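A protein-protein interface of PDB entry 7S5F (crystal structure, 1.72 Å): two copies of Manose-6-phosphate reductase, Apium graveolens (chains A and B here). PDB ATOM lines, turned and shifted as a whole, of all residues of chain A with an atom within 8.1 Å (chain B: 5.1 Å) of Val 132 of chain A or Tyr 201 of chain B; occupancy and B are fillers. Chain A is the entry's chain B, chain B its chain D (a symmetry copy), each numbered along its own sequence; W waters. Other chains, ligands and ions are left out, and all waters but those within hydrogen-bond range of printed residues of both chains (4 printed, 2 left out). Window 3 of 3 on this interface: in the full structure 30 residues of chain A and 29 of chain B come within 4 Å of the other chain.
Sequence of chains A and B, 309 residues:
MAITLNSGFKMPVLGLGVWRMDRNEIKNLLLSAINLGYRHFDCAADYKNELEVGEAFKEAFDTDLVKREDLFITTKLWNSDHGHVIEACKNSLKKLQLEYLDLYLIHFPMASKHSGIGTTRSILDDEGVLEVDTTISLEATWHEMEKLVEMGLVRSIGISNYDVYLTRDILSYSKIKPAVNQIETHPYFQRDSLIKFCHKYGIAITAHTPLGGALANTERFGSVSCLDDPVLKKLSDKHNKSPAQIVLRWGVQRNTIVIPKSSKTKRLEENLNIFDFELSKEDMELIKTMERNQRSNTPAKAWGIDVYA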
ATOM      1  N   ASN A  79      22.887  23.332  16.949  1.00  0.00           N
ATOM      2  CA  ASN A  79      22.359  21.971  17.027  1.00  0.00           C
ATOM      3  C   ASN A  79      23.437  20.939  17.315  1.00  0.00           C
ATOM      4  O   ASN A  79      23.148  19.891  17.894  1.00  0.00           O
ATOM      5  CB  ASN A  79      21.674  21.579  15.714  1.00  0.00           C
ATOM      6  CG  ASN A  79      20.614  22.572  15.273  1.00  0.00           C
ATOM      7  OD1 ASN A  79      20.248  23.480  16.016  1.00  0.00           O
ATOM      8  ND2 ASN A  79      20.095  22.379  14.060  1.00  0.00           N
ATOM      9  N   PRO A 109      15.156  23.446  18.053  1.00  0.00           N
ATOM     10  CA  PRO A 109      14.771  22.213  18.753  1.00  0.00           C
ATOM     11  C   PRO A 109      15.261  20.961  18.022  1.00  0.00           C
ATOM     12  O   PRO A 109      14.533  19.982  17.863  1.00  0.00           O
ATOM     13  CB  PRO A 109      13.244  22.307  18.782  1.00  0.00           C
ATOM     14  CG  PRO A 109      12.915  23.022  17.496  1.00  0.00           C
ATOM     15  CD  PRO A 109      14.009  24.060  17.352  1.00  0.00           C
ATOM     16  N   MET A 110      16.514  21.007  17.581  1.00  0.00           N
ATOM     17  CA  MET A 110      17.185  19.963  16.814  1.00  0.00           C
ATOM     18  C   MET A 110      18.572  19.732  17.384  1.00  0.00           C
ATOM     19  O   MET A 110      19.307  20.693  17.620  1.00  0.00           O
ATOM     20  CB  MET A 110      17.281  20.359  15.335  1.00  0.00           C
ATOM     21  CG  MET A 110      18.061  19.376  14.454  1.00  0.00           C
ATOM     22  SD  MET A 110      17.469  17.683  14.320  1.00  0.00           S
ATOM     23  CE  MET A 110      16.049  17.885  13.235  1.00  0.00           C
ATOM     24  N   ALA A 111      18.924  18.466  17.600  1.00  0.00           N
ATOM     25  CA  ALA A 111      20.288  18.074  17.920  1.00  0.00           C
ATOM     26  C   ALA A 111      20.837  17.256  16.764  1.00  0.00           C
ATOM     27  O   ALA A 111      20.162  16.339  16.278  1.00  0.00           O
ATOM     28  CB  ALA A 111      20.347  17.259  19.214  1.00  0.00           C
ATOM     29  N   SER A 112      22.052  17.586  16.326  1.00  0.00           N
ATOM     30  CA  SER A 112      22.727  16.839  15.276  1.00  0.00           C
ATOM     31  C   SER A 112      24.131  16.462  15.736  1.00  0.00           C
ATOM     32  O   SER A 112      24.587  16.874  16.803  1.00  0.00           O
ATOM     33  CB  SER A 112      22.786  17.632  13.959  1.00  0.00           C
ATOM     34  OG  SER A 112      23.433  18.885  14.127  1.00  0.00           O
ATOM     35  N   LYS A 113      24.814  15.674  14.906  1.00  0.00           N
ATOM     36  CA  LYS A 113      26.105  15.099  15.281  1.00  0.00           C
ATOM     37  C   LYS A 113      27.103  16.184  15.677  1.00  0.00           C
ATOM     38  O   LYS A 113      27.241  17.203  14.993  1.00  0.00           O
ATOM     39  CB  LYS A 113      26.655  14.268  14.118  1.00  0.00           C
ATOM     40  CG  LYS A 113      28.003  13.614  14.380  1.00  0.00           C
ATOM     41  CD  LYS A 113      28.403  12.729  13.206  1.00  0.00           C
ATOM     42  CE  LYS A 113      29.829  12.218  13.336  1.00  0.00           C
ATOM     43  NZ  LYS A 113      30.108  11.689  14.698  1.00  0.00           N
ATOM     44  N   HIS A 114      27.802  15.957  16.788  1.00  0.00           N
ATOM     45  CA  HIS A 114      28.760  16.934  17.286  1.00  0.00           C
ATOM     46  C   HIS A 114      29.917  17.097  16.305  1.00  0.00           C
ATOM     47  O   HIS A 114      30.458  16.117  15.780  1.00  0.00           O
ATOM     48  CB  HIS A 114      29.281  16.504  18.660  1.00  0.00           C
ATOM     49  CG  HIS A 114      30.257  17.461  19.274  1.00  0.00           C
ATOM     50  ND1 HIS A 114      29.909  18.739  19.652  1.00  0.00           N
ATOM     51  CD2 HIS A 114      31.566  17.317  19.594  1.00  0.00           C
ATOM     52  CE1 HIS A 114      30.963  19.348  20.166  1.00  0.00           C
ATOM     53  NE2 HIS A 114      31.983  18.507  20.144  1.00  0.00           N
ATOM     54  N   ILE A 123      26.414  18.316  10.045  1.00  0.00           N
ATOM     55  CA  ILE A 123      27.032  17.189   9.356  1.00  0.00           C
ATOM     56  C   ILE A 123      25.966  16.405   8.604  1.00  0.00           C
ATOM     57  O   ILE A 123      24.954  15.996   9.184  1.00  0.00           O
ATOM     58  CB  ILE A 123      27.762  16.289  10.365  1.00  0.00           C
ATOM     59  CG1 ILE A 123      28.917  17.042  11.027  1.00  0.00           C
ATOM     60  CG2 ILE A 123      28.251  15.009   9.697  1.00  0.00           C
ATOM     61  CD1 ILE A 123      29.520  16.311  12.215  1.00  0.00           C
ATOM     62  N   LEU A 124      26.191  16.186   7.313  1.00  0.00           N
ATOM     63  CA  LEU A 124      25.268  15.424   6.485  1.00  0.00           C
ATOM     64  C   LEU A 124      25.800  14.014   6.253  1.00  0.00           C
ATOM     65  O   LEU A 124      27.012  13.789   6.218  1.00  0.00           O
ATOM     66  CB  LEU A 124      25.043  16.116   5.139  1.00  0.00           C
ATOM     67  CG  LEU A 124      24.603  17.582   5.171  1.00  0.00           C
ATOM     68  CD1 LEU A 124      24.436  18.105   3.747  1.00  0.00           C
ATOM     69  CD2 LEU A 124      23.316  17.743   5.955  1.00  0.00           C
ATOM     70  N   ASP A 125      24.881  13.063   6.093  1.00  0.00           N
ATOM     71  CA  ASP A 125      25.296  11.722   5.719  1.00  0.00           C
ATOM     72  C   ASP A 125      25.579  11.674   4.219  1.00  0.00           C
ATOM     73  O   ASP A 125      25.469  12.676   3.508  1.00  0.00           O
ATOM     74  CB  ASP A 125      24.255  10.682   6.157  1.00  0.00           C
ATOM     75  CG  ASP A 125      22.921  10.787   5.411  1.00  0.00           C
ATOM     76  OD1 ASP A 125      22.836  11.381   4.317  1.00  0.00           O
ATOM     77  OD2 ASP A 125      21.930  10.225   5.925  1.00  0.00           O
ATOM     78  N   VAL A 129      21.555  13.955   3.982  1.00  0.00           N
ATOM     79  CA  VAL A 129      20.567  14.110   5.047  1.00  0.00           C
ATOM     80  C   VAL A 129      21.297  14.333   6.365  1.00  0.00           C
ATOM     81  O   VAL A 129      22.271  13.631   6.668  1.00  0.00           O
ATOM     82  CB  VAL A 129      19.637  12.889   5.129  1.00  0.00           C
ATOM     83  CG1 VAL A 129      18.614  13.055   6.258  1.00  0.00           C
ATOM     84  CG2 VAL A 129      18.942  12.668   3.789  1.00  0.00           C
ATOM     85  N   LEU A 130      20.818  15.307   7.144  1.00  0.00           N
ATOM     86  CA  LEU A 130      21.417  15.650   8.430  1.00  0.00           C
ATOM     87  C   LEU A 130      21.641  14.416   9.296  1.00  0.00           C
ATOM     88  O   LEU A 130      20.769  13.551   9.411  1.00  0.00           O
ATOM     89  CB  LEU A 130      20.514  16.644   9.168  1.00  0.00           C
ATOM     90  CG  LEU A 130      21.027  17.262  10.471  1.00  0.00           C
ATOM     91  CD1 LEU A 130      22.292  18.097  10.225  1.00  0.00           C
ATOM     92  CD2 LEU A 130      19.924  18.094  11.150  1.00  0.00           C
ATOM     93  N   GLU A 131      22.821  14.341   9.908  1.00  0.00           N
ATOM     94  CA  GLU A 131      23.122  13.298  10.885  1.00  0.00           C
ATOM     95  C   GLU A 131      22.441  13.695  12.185  1.00  0.00           C
ATOM     96  O   GLU A 131      23.027  14.365  13.036  1.00  0.00           O
ATOM     97  CB  GLU A 131      24.624  13.153  11.078  1.00  0.00           C
ATOM     98  CG  GLU A 131      25.341  12.446   9.954  1.00  0.00           C
ATOM     99  CD  GLU A 131      25.271  10.939  10.059  1.00  0.00           C
ATOM    100  OE1 GLU A 131      24.653  10.425  11.020  1.00  0.00           O
ATOM    101  OE2 GLU A 131      25.866  10.270   9.185  1.00  0.00           O
ATOM    102  N   VAL A 132      21.186  13.297  12.338  1.00  0.00           N
ATOM    103  CA  VAL A 132      20.401  13.729  13.486  1.00  0.00           C
ATOM    104  C   VAL A 132      20.836  12.940  14.715  1.00  0.00           C
ATOM    105  O   VAL A 132      21.097  11.731  14.645  1.00  0.00           O
ATOM    106  CB  VAL A 132      18.898  13.563  13.198  1.00  0.00           C
ATOM    107  CG1 VAL A 132      18.079  13.821  14.441  1.00  0.00           C
ATOM    108  CG2 VAL A 132      18.463  14.496  12.075  1.00  0.00           C
ATOM    109  N   ASP A 133      20.957  13.627  15.843  1.00  0.00           N
ATOM    110  CA  ASP A 133      21.267  12.962  17.096  1.00  0.00           C
ATOM    111  C   ASP A 133      19.972  12.524  17.769  1.00  0.00           C
ATOM    112  O   ASP A 133      19.005  13.288  17.832  1.00  0.00           O
ATOM    113  CB  ASP A 133      22.039  13.883  18.041  1.00  0.00           C
ATOM    114  CG  ASP A 133      22.087  13.337  19.463  1.00  0.00           C
ATOM    115  OD1 ASP A 133      21.186  13.648  20.264  1.00  0.00           O
ATOM    116  OD2 ASP A 133      23.020  12.573  19.770  1.00  0.00           O
ATOM    117  N   THR A 134      19.958  11.294  18.282  1.00  0.00           N
ATOM    118  CA  THR A 134      18.779  10.767  18.970  1.00  0.00           C
ATOM    119  C   THR A 134      19.152  10.272  20.358  1.00  0.00           C
ATOM    120  O   THR A 134      18.614   9.278  20.853  1.00  0.00           O
ATOM    121  CB  THR A 134      18.105   9.657  18.158  1.00  0.00           C
ATOM    122  OG1 THR A 134      19.057   8.640  17.823  1.00  0.00           O
ATOM    123  CG2 THR A 134      17.492  10.226  16.876  1.00  0.00           C
ATOM    124  N   THR A 135      20.098  10.955  21.001  1.00  0.00           N
ATOM    125  CA  THR A 135      20.505  10.622  22.356  1.00  0.00           C
ATOM    126  C   THR A 135      20.276  11.742  23.360  1.00  0.00           C
ATOM    127  O   THR A 135      20.150  11.454  24.554  1.00  0.00           O
ATOM    128  CB  THR A 135      21.993  10.231  22.398  1.00  0.00           C
ATOM    129  OG1 THR A 135      22.802  11.394  22.189  1.00  0.00           O
ATOM    130  CG2 THR A 135      22.318   9.199  21.331  1.00  0.00           C
ATOM    131  N   TRP A 303      19.544  20.944   5.563  1.00  0.00           N
ATOM    132  CA  TRP A 303      19.572  19.710   6.329  1.00  0.00           C
ATOM    133  C   TRP A 303      19.084  18.501   5.545  1.00  0.00           C
ATOM    134  O   TRP A 303      19.246  17.374   6.021  1.00  0.00           O
ATOM    135  CB  TRP A 303      18.732  19.856   7.606  1.00  0.00           C
ATOM    136  CG  TRP A 303      19.161  20.977   8.493  1.00  0.00           C
ATOM    137  CD1 TRP A 303      20.314  21.711   8.400  1.00  0.00           C
ATOM    138  CD2 TRP A 303      18.446  21.497   9.617  1.00  0.00           C
ATOM    139  NE1 TRP A 303      20.351  22.659   9.394  1.00  0.00           N
ATOM    140  CE2 TRP A 303      19.218  22.549  10.156  1.00  0.00           C
ATOM    141  CE3 TRP A 303      17.231  21.175  10.222  1.00  0.00           C
ATOM    142  CZ2 TRP A 303      18.806  23.285  11.273  1.00  0.00           C
ATOM    143  CZ3 TRP A 303      16.819  21.910  11.327  1.00  0.00           C
ATOM    144  CH2 TRP A 303      17.605  22.951  11.839  1.00  0.00           C
ATOM    145  N   ILE A 305      16.110  17.665   5.190  1.00  0.00           N
ATOM    146  CA  ILE A 305      14.918  17.217   5.902  1.00  0.00           C
ATOM    147  C   ILE A 305      13.979  18.408   6.010  1.00  0.00           C
ATOM    148  O   ILE A 305      14.355  19.442   6.572  1.00  0.00           O
ATOM    149  CB  ILE A 305      15.239  16.694   7.315  1.00  0.00           C
ATOM    150  CG1 ILE A 305      16.191  15.500   7.272  1.00  0.00           C
ATOM    151  CG2 ILE A 305      13.941  16.354   8.067  1.00  0.00           C
ATOM    152  CD1 ILE A 305      16.702  15.092   8.659  1.00  0.00           C
ATOM    153  N   VAL A 307      11.838  19.798   8.131  1.00  0.00           N
ATOM    154  CA  VAL A 307      11.419  19.698   9.521  1.00  0.00           C
ATOM    155  C   VAL A 307      10.004  20.216   9.735  1.00  0.00           C
ATOM    156  O   VAL A 307       9.399  19.940  10.774  1.00  0.00           O
ATOM    157  CB  VAL A 307      12.417  20.448  10.422  1.00  0.00           C
ATOM    158  CG1 VAL A 307      13.738  19.700  10.468  1.00  0.00           C
ATOM    159  CG2 VAL A 307      12.611  21.882   9.919  1.00  0.00           C
ATOM    160  N   ASN B   6       8.589  -2.559  15.806  1.00  0.00           N
ATOM    161  CA  ASN B   6       9.829  -2.758  16.547  1.00  0.00           C
ATOM    162  C   ASN B   6       9.594  -3.454  17.882  1.00  0.00           C
ATOM    163  O   ASN B   6      10.558  -3.904  18.507  1.00  0.00           O
ATOM    164  CB  ASN B   6      10.561  -1.421  16.751  1.00  0.00           C
ATOM    165  CG  ASN B   6       9.691  -0.358  17.405  1.00  0.00           C
ATOM    166  OD1 ASN B   6       8.601  -0.639  17.905  1.00  0.00           O
ATOM    167  ND2 ASN B   6      10.182   0.876  17.416  1.00  0.00           N
ATOM    168  N   ARG B 168      12.192  13.200  17.179  1.00  0.00           N
ATOM    169  CA  ARG B 168      13.588  13.121  17.594  1.00  0.00           C
ATOM    170  C   ARG B 168      13.705  13.162  19.109  1.00  0.00           C
ATOM    171  O   ARG B 168      14.537  12.461  19.700  1.00  0.00           O
ATOM    172  CB  ARG B 168      14.396  14.260  16.981  1.00  0.00           C
ATOM    173  CG  ARG B 168      15.909  14.079  17.156  1.00  0.00           C
ATOM    174  CD  ARG B 168      16.670  15.397  17.304  1.00  0.00           C
ATOM    175  NE  ARG B 168      16.303  16.091  18.529  1.00  0.00           N
ATOM    176  CZ  ARG B 168      16.814  15.823  19.723  1.00  0.00           C
ATOM    177  NH1 ARG B 168      17.785  14.936  19.879  1.00  0.00           N
ATOM    178  NH2 ARG B 168      16.331  16.451  20.789  1.00  0.00           N
ATOM    179  N   LEU B 171      12.645   9.859  20.646  1.00  0.00           N
ATOM    180  CA  LEU B 171      13.707   8.893  20.390  1.00  0.00           C
ATOM    181  C   LEU B 171      14.857   9.069  21.378  1.00  0.00           C
ATOM    182  O   LEU B 171      15.497   8.088  21.771  1.00  0.00           O
ATOM    183  CB  LEU B 171      14.206   9.024  18.952  1.00  0.00           C
ATOM    184  CG  LEU B 171      13.312   8.432  17.853  1.00  0.00           C
ATOM    185  CD1 LEU B 171      13.741   8.945  16.480  1.00  0.00           C
ATOM    186  CD2 LEU B 171      13.345   6.897  17.890  1.00  0.00           C
ATOM    187  N   PHE B 197      12.006   9.970   8.065  1.00  0.00           N
ATOM    188  CA  PHE B 197      12.658  10.094   9.363  1.00  0.00           C
ATOM    189  C   PHE B 197      12.194   9.002  10.316  1.00  0.00           C
ATOM    190  O   PHE B 197      13.007   8.325  10.955  1.00  0.00           O
ATOM    191  CB  PHE B 197      12.368  11.478   9.949  1.00  0.00           C
ATOM    192  CG  PHE B 197      13.044  11.736  11.262  1.00  0.00           C
ATOM    193  CD1 PHE B 197      14.379  12.106  11.309  1.00  0.00           C
ATOM    194  CD2 PHE B 197      12.335  11.632  12.455  1.00  0.00           C
ATOM    195  CE1 PHE B 197      15.003  12.355  12.516  1.00  0.00           C
ATOM    196  CE2 PHE B 197      12.954  11.877  13.667  1.00  0.00           C
ATOM    197  CZ  PHE B 197      14.289  12.241  13.700  1.00  0.00           C
ATOM    198  N   CYS B 198      10.883   8.811  10.414  1.00  0.00           N
ATOM    199  CA  CYS B 198      10.348   7.793  11.306  1.00  0.00           C
ATOM    200  C   CYS B 198      10.828   6.408  10.888  1.00  0.00           C
ATOM    201  O   CYS B 198      11.271   5.608  11.723  1.00  0.00           O
ATOM    202  CB  CYS B 198       8.824   7.877  11.307  1.00  0.00           C
ATOM    203  SG  CYS B 198       8.225   9.311  12.234  1.00  0.00           S
ATOM    204  N   HIS B 199      10.779   6.121   9.584  1.00  0.00           N
ATOM    205  CA  HIS B 199      11.200   4.813   9.100  1.00  0.00           C
ATOM    206  C   HIS B 199      12.679   4.575   9.353  1.00  0.00           C
ATOM    207  O   HIS B 199      13.091   3.444   9.647  1.00  0.00           O
ATOM    208  CB  HIS B 199      10.879   4.689   7.614  1.00  0.00           C
ATOM    209  CG  HIS B 199       9.442   4.392   7.332  1.00  0.00           C
ATOM    210  ND1 HIS B 199       8.925   4.364   6.055  1.00  0.00           N
ATOM    211  CD2 HIS B 199       8.414   4.089   8.161  1.00  0.00           C
ATOM    212  CE1 HIS B 199       7.640   4.053   6.110  1.00  0.00           C
ATOM    213  NE2 HIS B 199       7.305   3.885   7.376  1.00  0.00           N
ATOM    214  N   LYS B 200      13.496   5.627   9.235  1.00  0.00           N
ATOM    215  CA  LYS B 200      14.927   5.482   9.459  1.00  0.00           C
ATOM    216  C   LYS B 200      15.212   4.945  10.850  1.00  0.00           C
ATOM    217  O   LYS B 200      16.189   4.209  11.048  1.00  0.00           O
ATOM    218  CB  LYS B 200      15.624   6.826   9.258  1.00  0.00           C
ATOM    219  CG  LYS B 200      17.129   6.780   9.452  1.00  0.00           C
ATOM    220  CD  LYS B 200      17.765   8.139   9.184  1.00  0.00           C
ATOM    221  CE  LYS B 200      19.278   8.074   9.326  1.00  0.00           C
ATOM    222  NZ  LYS B 200      19.875   7.154   8.319  1.00  0.00           N
ATOM    223  N   TYR B 201      14.359   5.281  11.813  1.00  0.00           N
ATOM    224  CA  TYR B 201      14.543   4.881  13.197  1.00  0.00           C
ATOM    225  C   TYR B 201      13.599   3.763  13.615  1.00  0.00           C
ATOM    226  O   TYR B 201      13.438   3.516  14.814  1.00  0.00           O
ATOM    227  CB  TYR B 201      14.382   6.110  14.091  1.00  0.00           C
ATOM    228  CG  TYR B 201      15.554   7.036  13.917  1.00  0.00           C
ATOM    229  CD1 TYR B 201      16.801   6.702  14.437  1.00  0.00           C
ATOM    230  CD2 TYR B 201      15.430   8.218  13.189  1.00  0.00           C
ATOM    231  CE1 TYR B 201      17.887   7.529  14.269  1.00  0.00           C
ATOM    232  CE2 TYR B 201      16.515   9.052  13.007  1.00  0.00           C
ATOM    233  CZ  TYR B 201      17.742   8.700  13.549  1.00  0.00           C
ATOM    234  OH  TYR B 201      18.831   9.521  13.385  1.00  0.00           O
ATOM    235  N   GLY B 202      12.988   3.070  12.659  1.00  0.00           N
ATOM    236  CA  GLY B 202      12.202   1.895  12.956  1.00  0.00           C
ATOM    237  C   GLY B 202      10.808   2.159  13.472  1.00  0.00           C
ATOM    238  O   GLY B 202      10.167   1.233  13.978  1.00  0.00           O
ATOM    239  N   ILE B 203      10.317   3.389  13.358  1.00  0.00           N
ATOM    240  CA  ILE B 203       8.972   3.732  13.797  1.00  0.00           C
ATOM    241  C   ILE B 203       8.031   3.550  12.618  1.00  0.00           C
ATOM    242  O   ILE B 203       8.242   4.140  11.554  1.00  0.00           O
ATOM    243  CB  ILE B 203       8.908   5.173  14.327  1.00  0.00           C
ATOM    244  CG1 ILE B 203       9.873   5.372  15.499  1.00  0.00           C
ATOM    245  CG2 ILE B 203       7.486   5.523  14.738  1.00  0.00           C
ATOM    246  CD1 ILE B 203      10.106   6.836  15.838  1.00  0.00           C
HETATM  247  O   HOH W   1      20.659   8.774  15.646  1.00  0.00           O
HETATM  248  O   HOH W   2      22.364   7.828   7.178  1.00  0.00           O
HETATM  249  O   HOH W   3      18.331   6.744  21.755  1.00  0.00           O
HETATM  250  O   HOH W   4      14.055  17.545  18.972  1.00  0.00           O
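The side-chain hydroxyl (OH) of Tyr 201 of chain B lies within hydrogen-bond range of the backbone carbonyl oxygen (O) of Val 132 of chain A, 3.4 Å away. The side-chain carboxylate (OD1) of Asp 133 of chain A is in salt-bridge range of the guanidinium group (NH1) of Arg 168 of chain B (3.7 Å). O of Leu 171 of chain B lies close to O of Thr 134 of chain A, at 3.5 Å.
OD1 of Asn 79 of chain A sits close to O of Met 110 of chain A, at 3.4 Å. N of Asp 133 of chain A sits at hydrogen-bond distance from O of Ala 111 of chain A, 2.9 Å away. The side-chain carboxylate (OD2) of Asp 133 of chain A sits at hydrogen-bond distance from the side-chain hydroxyl (OG1) of Thr 135 of chain A (2.7 Å).
Among the printed residues, pairs that only touch across the chains: Met 110 of chain A with Arg 168 of chain B, Ala 111 of chain A with Arg 168 of chain B, Val 132 of chain A with Arg 168 of chain B, Val 132 of chain A with Phe 197 of chain B and Thr 134 of chain A with Tyr 201 of chain B.
Ile 123 of chain A touches none of the printed residues of chain B. Val 129 of chain A touches none of the printed residues of chain B. Of chain B, only Arg 168, Phe 197 and Tyr 201 come within 4 Å of Val 132 of chain A. Printed residues of chain B within 4 Å of Asp 133 of chain A: Arg 168 (2.9 Å). Of the printed residues of chain A, Arg 168 of chain B touches Met 110, Ala 111, Val 132 and Asp 133. Of chain A, only Val 132 and Thr 134 come within 4 Å of Tyr 201 of chain B. The nearest printed residue of chain B that does not touch Val 132 of chain A is Lys 200 of chain B (6.3 Å). The nearest residue of chain A that does not touch Tyr 201 of chain B is Asp 133 of chain A (5.2 Å). The nearest printed residue of chain B that does not touch Thr 134 of chain A is Arg 168 of chain B (4.2 Å).
Of the 20 printed residues of chain A, 5 touch a printed residue of chain B. Printed residues of chain A that touch a printed residue of chain B: Met 110, Ala 111, Val 132, Asp 133 and Thr 134. Hydrophobic or aromatic side chains of chain A within 4 Å of the printed part of chain B: Met 110, Ala 111 and Val 132. Hydrophobic or aromatic side chains of chain B within 4 Å of the printed part of chain A: Leu 171, Phe 197 and Tyr 201. Among the printed residues, 8 pairs touch across the chains. Among the printed residues, Asp or Glu carboxylates within 4 Å of a Lys or Arg side-chain nitrogen of the other chain: Asp 133 of chain A with Arg 168 of chain B (3.7 Å).
No position is printed for both chains. Of the 8 pairs that touch across the chains among the printed residues, none has its exchanged pair printed and touching as well.
Water W3 lies within hydrogen-bond range of O of Thr 134 of chain A (2.7 Å) and O of Leu 171 of chain B (3.1 Å). Water W1 lies within hydrogen-bond range of the side-chain hydroxyl (OG1) of Thr 134 of chain A (2.7 Å), the side-chain hydroxyl (OH) of Tyr 201 of chain B (3.0 Å) and the backbone carbonyl oxygen (O) of Val 132 of chain A (3.2 Å). Water W4 bridges the guanidinium group of Arg 168 of chain B (2.7 Å) and the backbone carbonyl oxygen of Pro 109 of chain A (2.7 Å). Water W2 bridges OD2 of Asp 125 of chain A (2.7 Å) and NZ of Lys 200 of chain B (2.8 Å).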
